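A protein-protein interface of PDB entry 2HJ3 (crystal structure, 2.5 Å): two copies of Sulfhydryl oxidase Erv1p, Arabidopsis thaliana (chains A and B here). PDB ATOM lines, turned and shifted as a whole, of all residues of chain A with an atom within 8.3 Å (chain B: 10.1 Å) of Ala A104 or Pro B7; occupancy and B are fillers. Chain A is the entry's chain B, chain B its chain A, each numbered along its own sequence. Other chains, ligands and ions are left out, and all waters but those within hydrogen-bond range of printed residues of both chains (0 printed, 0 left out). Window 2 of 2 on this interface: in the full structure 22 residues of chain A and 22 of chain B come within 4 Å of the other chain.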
ATOM      1  N   THR A  19      24.688 -23.942 -28.700  1.00  0.00           N
ATOM      2  CA  THR A  19      23.903 -23.529 -27.547  1.00  0.00           C
ATOM      3  C   THR A  19      22.733 -24.489 -27.383  1.00  0.00           C
ATOM      4  O   THR A  19      22.399 -24.883 -26.272  1.00  0.00           O
ATOM      5  CB  THR A  19      23.363 -22.094 -27.712  1.00  0.00           C
ATOM      6  OG1 THR A  19      24.464 -21.180 -27.788  1.00  0.00           O
ATOM      7  CG2 THR A  19      22.484 -21.711 -26.530  1.00  0.00           C
ATOM      8  N   THR A  23      22.764 -27.326 -24.378  1.00  0.00           N
ATOM      9  CA  THR A  23      21.706 -27.144 -23.393  1.00  0.00           C
ATOM     10  C   THR A  23      20.902 -28.439 -23.357  1.00  0.00           C
ATOM     11  O   THR A  23      20.479 -28.896 -22.294  1.00  0.00           O
ATOM     12  CB  THR A  23      20.774 -25.984 -23.759  1.00  0.00           C
ATOM     13  OG1 THR A  23      21.551 -24.804 -23.979  1.00  0.00           O
ATOM     14  CG2 THR A  23      19.778 -25.726 -22.628  1.00  0.00           C
ATOM     15  N   ALA A  26      22.691 -30.823 -21.365  1.00  0.00           N
ATOM     16  CA  ALA A  26      22.715 -30.461 -19.942  1.00  0.00           C
ATOM     17  C   ALA A  26      21.409 -30.861 -19.250  1.00  0.00           C
ATOM     18  O   ALA A  26      21.367 -31.019 -18.029  1.00  0.00           O
ATOM     19  CB  ALA A  26      22.947 -28.953 -19.778  1.00  0.00           C
ATOM     20  N   GLN A  27      20.350 -31.027 -20.037  1.00  0.00           N
ATOM     21  CA  GLN A  27      19.035 -31.389 -19.510  1.00  0.00           C
ATOM     22  C   GLN A  27      18.688 -32.868 -19.726  1.00  0.00           C
ATOM     23  O   GLN A  27      17.637 -33.343 -19.289  1.00  0.00           O
ATOM     24  CB  GLN A  27      17.970 -30.510 -20.166  1.00  0.00           C
ATOM     25  CG  GLN A  27      18.153 -29.027 -19.894  1.00  0.00           C
ATOM     26  CD  GLN A  27      17.635 -28.621 -18.529  1.00  0.00           C
ATOM     27  OE1 GLN A  27      16.440 -28.735 -18.251  1.00  0.00           O
ATOM     28  NE2 GLN A  27      18.530 -28.140 -17.670  1.00  0.00           N
ATOM     29  N   PHE A  97      38.254 -26.339 -25.116  1.00  0.00           N
ATOM     30  CA  PHE A  97      37.455 -26.255 -23.902  1.00  0.00           C
ATOM     31  C   PHE A  97      37.684 -27.487 -23.014  1.00  0.00           C
ATOM     32  O   PHE A  97      37.454 -28.616 -23.442  1.00  0.00           O
ATOM     33  CB  PHE A  97      35.982 -26.159 -24.328  1.00  0.00           C
ATOM     34  CG  PHE A  97      35.003 -26.031 -23.190  1.00  0.00           C
ATOM     35  CD1 PHE A  97      34.533 -24.781 -22.797  1.00  0.00           C
ATOM     36  CD2 PHE A  97      34.533 -27.163 -22.527  1.00  0.00           C
ATOM     37  CE1 PHE A  97      33.605 -24.661 -21.763  1.00  0.00           C
ATOM     38  CE2 PHE A  97      33.607 -27.055 -21.491  1.00  0.00           C
ATOM     39  CZ  PHE A  97      33.142 -25.804 -21.107  1.00  0.00           C
ATOM     40  N   PRO A  98      38.155 -27.288 -21.772  1.00  0.00           N
ATOM     41  CA  PRO A  98      38.384 -28.437 -20.887  1.00  0.00           C
ATOM     42  C   PRO A  98      37.040 -29.092 -20.569  1.00  0.00           C
ATOM     43  O   PRO A  98      36.161 -28.467 -19.983  1.00  0.00           O
ATOM     44  CB  PRO A  98      39.051 -27.804 -19.664  1.00  0.00           C
ATOM     45  CG  PRO A  98      38.440 -26.437 -19.628  1.00  0.00           C
ATOM     46  CD  PRO A  98      38.477 -26.026 -21.087  1.00  0.00           C
ATOM     47  N   GLU A 100      35.501 -30.736 -18.362  1.00  0.00           N
ATOM     48  CA  GLU A 100      35.034 -31.047 -17.017  1.00  0.00           C
ATOM     49  C   GLU A 100      34.137 -29.848 -16.717  1.00  0.00           C
ATOM     50  O   GLU A 100      33.271 -29.876 -15.841  1.00  0.00           O
ATOM     51  CB  GLU A 100      36.200 -31.103 -16.024  1.00  0.00           C
ATOM     52  CG  GLU A 100      37.461 -31.802 -16.530  1.00  0.00           C
ATOM     53  CD  GLU A 100      37.215 -33.212 -17.038  1.00  0.00           C
ATOM     54  OE1 GLU A 100      38.207 -33.949 -17.235  1.00  0.00           O
ATOM     55  OE2 GLU A 100      36.040 -33.583 -17.250  1.00  0.00           O
ATOM     56  N   ARG A 101      34.358 -28.810 -17.517  1.00  0.00           N
ATOM     57  CA  ARG A 101      33.672 -27.529 -17.447  1.00  0.00           C
ATOM     58  C   ARG A 101      32.379 -27.446 -18.286  1.00  0.00           C
ATOM     59  O   ARG A 101      31.824 -26.360 -18.458  1.00  0.00           O
ATOM     60  CB  ARG A 101      34.674 -26.449 -17.891  1.00  0.00           C
ATOM     61  CG  ARG A 101      34.137 -25.037 -18.090  1.00  0.00           C
ATOM     62  CD  ARG A 101      35.147 -24.168 -18.855  1.00  0.00           C
ATOM     63  NE  ARG A 101      34.620 -22.837 -19.159  1.00  0.00           N
ATOM     64  CZ  ARG A 101      35.300 -21.880 -19.788  1.00  0.00           C
ATOM     65  NH1 ARG A 101      36.549 -22.095 -20.186  1.00  0.00           N
ATOM     66  NH2 ARG A 101      34.728 -20.706 -20.025  1.00  0.00           N
ATOM     67  N   VAL A 102      31.887 -28.571 -18.801  1.00  0.00           N
ATOM     68  CA  VAL A 102      30.666 -28.524 -19.611  1.00  0.00           C
ATOM     69  C   VAL A 102      29.464 -28.029 -18.810  1.00  0.00           C
ATOM     70  O   VAL A 102      28.733 -27.145 -19.261  1.00  0.00           O
ATOM     71  CB  VAL A 102      30.312 -29.899 -20.233  1.00  0.00           C
ATOM     72  CG1 VAL A 102      31.437 -30.363 -21.124  1.00  0.00           C
ATOM     73  CG2 VAL A 102      30.031 -30.921 -19.149  1.00  0.00           C
ATOM     74  N   ASP A 103      29.263 -28.588 -17.619  1.00  0.00           N
ATOM     75  CA  ASP A 103      28.143 -28.178 -16.780  1.00  0.00           C
ATOM     76  C   ASP A 103      28.348 -26.748 -16.286  1.00  0.00           C
ATOM     77  O   ASP A 103      27.648 -26.285 -15.386  1.00  0.00           O
ATOM     78  CB  ASP A 103      27.983 -29.129 -15.588  1.00  0.00           C
ATOM     79  CG  ASP A 103      27.748 -30.568 -16.013  1.00  0.00           C
ATOM     80  OD1 ASP A 103      26.936 -30.794 -16.936  1.00  0.00           O
ATOM     81  OD2 ASP A 103      28.366 -31.475 -15.420  1.00  0.00           O
ATOM     82  N   ALA A 104      29.313 -26.057 -16.891  1.00  0.00           N
ATOM     83  CA  ALA A 104      29.643 -24.675 -16.545  1.00  0.00           C
ATOM     84  C   ALA A 104      29.023 -23.722 -17.545  1.00  0.00           C
ATOM     85  O   ALA A 104      28.184 -22.887 -17.202  1.00  0.00           O
ATOM     86  CB  ALA A 104      31.161 -24.483 -16.538  1.00  0.00           C
ATOM     87  N   ARG A 105      29.463 -23.849 -18.789  1.00  0.00           N
ATOM     88  CA  ARG A 105      28.970 -23.009 -19.859  1.00  0.00           C
ATOM     89  C   ARG A 105      27.494 -23.302 -20.123  1.00  0.00           C
ATOM     90  O   ARG A 105      26.789 -22.474 -20.702  1.00  0.00           O
ATOM     91  CB  ARG A 105      29.794 -23.254 -21.128  1.00  0.00           C
ATOM     92  CG  ARG A 105      29.355 -22.420 -22.309  1.00  0.00           C
ATOM     93  CD  ARG A 105      29.557 -20.947 -22.044  1.00  0.00           C
ATOM     94  NE  ARG A 105      28.575 -20.133 -22.753  1.00  0.00           N
ATOM     95  CZ  ARG A 105      28.597 -18.805 -22.792  1.00  0.00           C
ATOM     96  NH1 ARG A 105      29.560 -18.137 -22.164  1.00  0.00           N
ATOM     97  NH2 ARG A 105      27.651 -18.144 -23.445  1.00  0.00           N
ATOM     98  N   TRP A 106      27.032 -24.469 -19.674  1.00  0.00           N
ATOM     99  CA  TRP A 106      25.647 -24.893 -19.892  1.00  0.00           C
ATOM    100  C   TRP A 106      24.868 -25.202 -18.613  1.00  0.00           C
ATOM    101  O   TRP A 106      24.583 -26.394 -18.366  1.00  0.00           O
ATOM    102  CB  TRP A 106      25.631 -26.113 -20.820  1.00  0.00           C
ATOM    103  CG  TRP A 106      26.589 -25.964 -21.954  1.00  0.00           C
ATOM    104  CD1 TRP A 106      27.661 -26.759 -22.230  1.00  0.00           C
ATOM    105  CD2 TRP A 106      26.622 -24.897 -22.912  1.00  0.00           C
ATOM    106  NE1 TRP A 106      28.368 -26.250 -23.294  1.00  0.00           N
ATOM    107  CE2 TRP A 106      27.751 -25.107 -23.732  1.00  0.00           C
ATOM    108  CE3 TRP A 106      25.807 -23.779 -23.155  1.00  0.00           C
ATOM    109  CZ2 TRP A 106      28.089 -24.240 -24.781  1.00  0.00           C
ATOM    110  CZ3 TRP A 106      26.146 -22.918 -24.198  1.00  0.00           C
ATOM    111  CH2 TRP A 106      27.277 -23.156 -24.997  1.00  0.00           C
ATOM    112  N   PRO B   7      23.494 -19.614 -16.607  1.00  0.00           N
ATOM    113  CA  PRO B   7      23.803 -19.339 -18.031  1.00  0.00           C
ATOM    114  C   PRO B   7      22.699 -19.884 -18.937  1.00  0.00           C
ATOM    115  O   PRO B   7      22.012 -20.845 -18.581  1.00  0.00           O
ATOM    116  CB  PRO B   7      25.129 -20.021 -18.328  1.00  0.00           C
ATOM    117  CG  PRO B   7      25.087 -21.188 -17.333  1.00  0.00           C
ATOM    118  CD  PRO B   7      24.471 -20.574 -16.060  1.00  0.00           C
ATOM    119  N   VAL B   8      22.535 -19.270 -20.106  1.00  0.00           N
ATOM    120  CA  VAL B   8      21.520 -19.697 -21.064  1.00  0.00           C
ATOM    121  C   VAL B   8      20.126 -19.802 -20.444  1.00  0.00           C
ATOM    122  O   VAL B   8      19.791 -20.793 -19.794  1.00  0.00           O
ATOM    123  CB  VAL B   8      21.901 -21.062 -21.704  1.00  0.00           C
ATOM    124  CG1 VAL B   8      20.730 -21.619 -22.501  1.00  0.00           C
ATOM    125  CG2 VAL B   8      23.103 -20.883 -22.622  1.00  0.00           C
ATOM    126  N   THR B   9      19.319 -18.767 -20.654  1.00  0.00           N
ATOM    127  CA  THR B   9      17.959 -18.734 -20.136  1.00  0.00           C
ATOM    128  C   THR B   9      17.009 -19.319 -21.175  1.00  0.00           C
ATOM    129  O   THR B   9      17.416 -19.655 -22.285  1.00  0.00           O
ATOM    130  CB  THR B   9      17.507 -17.287 -19.830  1.00  0.00           C
ATOM    131  OG1 THR B   9      17.539 -16.509 -21.035  1.00  0.00           O
ATOM    132  CG2 THR B   9      18.425 -16.645 -18.804  1.00  0.00           C
ATOM    133  N   LYS B  10      15.744 -19.442 -20.799  1.00  0.00           N
ATOM    134  CA  LYS B  10      14.720 -19.959 -21.691  1.00  0.00           C
ATOM    135  C   LYS B  10      14.745 -19.160 -22.995  1.00  0.00           C
ATOM    136  O   LYS B  10      14.543 -19.709 -24.081  1.00  0.00           O
ATOM    137  CB  LYS B  10      13.351 -19.821 -21.025  1.00  0.00           C
ATOM    138  CG  LYS B  10      12.176 -20.127 -21.927  1.00  0.00           C
ATOM    139  CD  LYS B  10      10.875 -19.555 -21.359  1.00  0.00           C
ATOM    140  CE  LYS B  10      10.509 -20.180 -20.018  1.00  0.00           C
ATOM    141  NZ  LYS B  10       9.174 -19.711 -19.533  1.00  0.00           N
ATOM    142  N   GLU B  11      15.005 -17.860 -22.879  1.00  0.00           N
ATOM    143  CA  GLU B  11      15.047 -16.986 -24.045  1.00  0.00           C
ATOM    144  C   GLU B  11      16.268 -17.211 -24.926  1.00  0.00           C
ATOM    145  O   GLU B  11      16.153 -17.188 -26.149  1.00  0.00           O
ATOM    146  CB  GLU B  11      14.986 -15.514 -23.622  1.00  0.00           C
ATOM    147  CG  GLU B  11      13.686 -15.086 -22.939  1.00  0.00           C
ATOM    148  CD  GLU B  11      13.574 -15.590 -21.506  1.00  0.00           C
ATOM    149  OE1 GLU B  11      14.590 -15.534 -20.778  1.00  0.00           O
ATOM    150  OE2 GLU B  11      12.474 -16.024 -21.098  1.00  0.00           O
ATOM    151  N   ASP B  12      17.435 -17.419 -24.319  1.00  0.00           N
ATOM    152  CA  ASP B  12      18.651 -17.653 -25.095  1.00  0.00           C
ATOM    153  C   ASP B  12      18.518 -18.950 -25.889  1.00  0.00           C
ATOM    154  O   ASP B  12      18.954 -19.032 -27.040  1.00  0.00           O
ATOM    155  CB  ASP B  12      19.880 -17.742 -24.185  1.00  0.00           C
ATOM    156  CG  ASP B  12      20.243 -16.408 -23.544  1.00  0.00           C
ATOM    157  OD1 ASP B  12      20.493 -15.431 -24.283  1.00  0.00           O
ATOM    158  OD2 ASP B  12      20.287 -16.343 -22.295  1.00  0.00           O
ATOM    159  N   LEU B  13      17.918 -19.962 -25.266  1.00  0.00           N
ATOM    160  CA  LEU B  13      17.722 -21.255 -25.909  1.00  0.00           C
ATOM    161  C   LEU B  13      16.809 -21.058 -27.112  1.00  0.00           C
ATOM    162  O   LEU B  13      17.132 -21.473 -28.226  1.00  0.00           O
ATOM    163  CB  LEU B  13      17.088 -22.248 -24.928  1.00  0.00           C
ATOM    164  CG  LEU B  13      16.916 -23.687 -25.430  1.00  0.00           C
ATOM    165  CD1 LEU B  13      18.283 -24.309 -25.614  1.00  0.00           C
ATOM    166  CD2 LEU B  13      16.088 -24.506 -24.454  1.00  0.00           C
ATOM    167  N   PRO B  52      14.849 -28.720 -24.457  1.00  0.00           N
ATOM    168  CA  PRO B  52      15.306 -28.392 -23.096  1.00  0.00           C
ATOM    169  C   PRO B  52      14.523 -27.422 -22.211  1.00  0.00           C
ATOM    170  O   PRO B  52      15.074 -26.917 -21.241  1.00  0.00           O
ATOM    171  CB  PRO B  52      16.737 -27.909 -23.316  1.00  0.00           C
ATOM    172  CG  PRO B  52      17.160 -28.648 -24.526  1.00  0.00           C
ATOM    173  CD  PRO B  52      15.952 -28.533 -25.416  1.00  0.00           C
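No position is printed for both chains.
Of the 7 pairs that touch across the chains among the printed residues, none has its exchanged pair printed and touching as well.
Printed residues of chain B that touch a printed residue of chain A: Pro B7, Val B8, Leu B13 and Pro B52.
Among the printed residues, 7 pairs touch across the chains.
Printed residues of chain B within 4 Å of Ala A104: Pro B7 (3.5 Å).
Printed residues of chain B within 4 Å of Trp A106: Val B8.
Pro B7 touches two residues of chain A.
Printed residues of chain A within 4 Å of Pro B52: Thr A23 (3.8 Å) and Gln A27 (3.8 Å).
The nearest residue of chain B that does not touch Ala A104 is Val B8 (7.3 Å).
The nearest residue of chain A that does not touch Pro B7 is Trp A106 (4.2 Å).
Among the printed residues, pairs that only touch across the chains: Thr A23 with Leu B13, Ala A104 with Pro B7, Thr A23 with Val B8, Gln A27 with Pro B52, Arg A105 with Pro B7, Thr A23 with Pro B52 and Trp A106 with Val B8.
The side-chain hydroxyl of Thr A23 is in hydrogen-bond range of the backbone carbonyl oxygen of Thr A19, at 2.4 Å.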
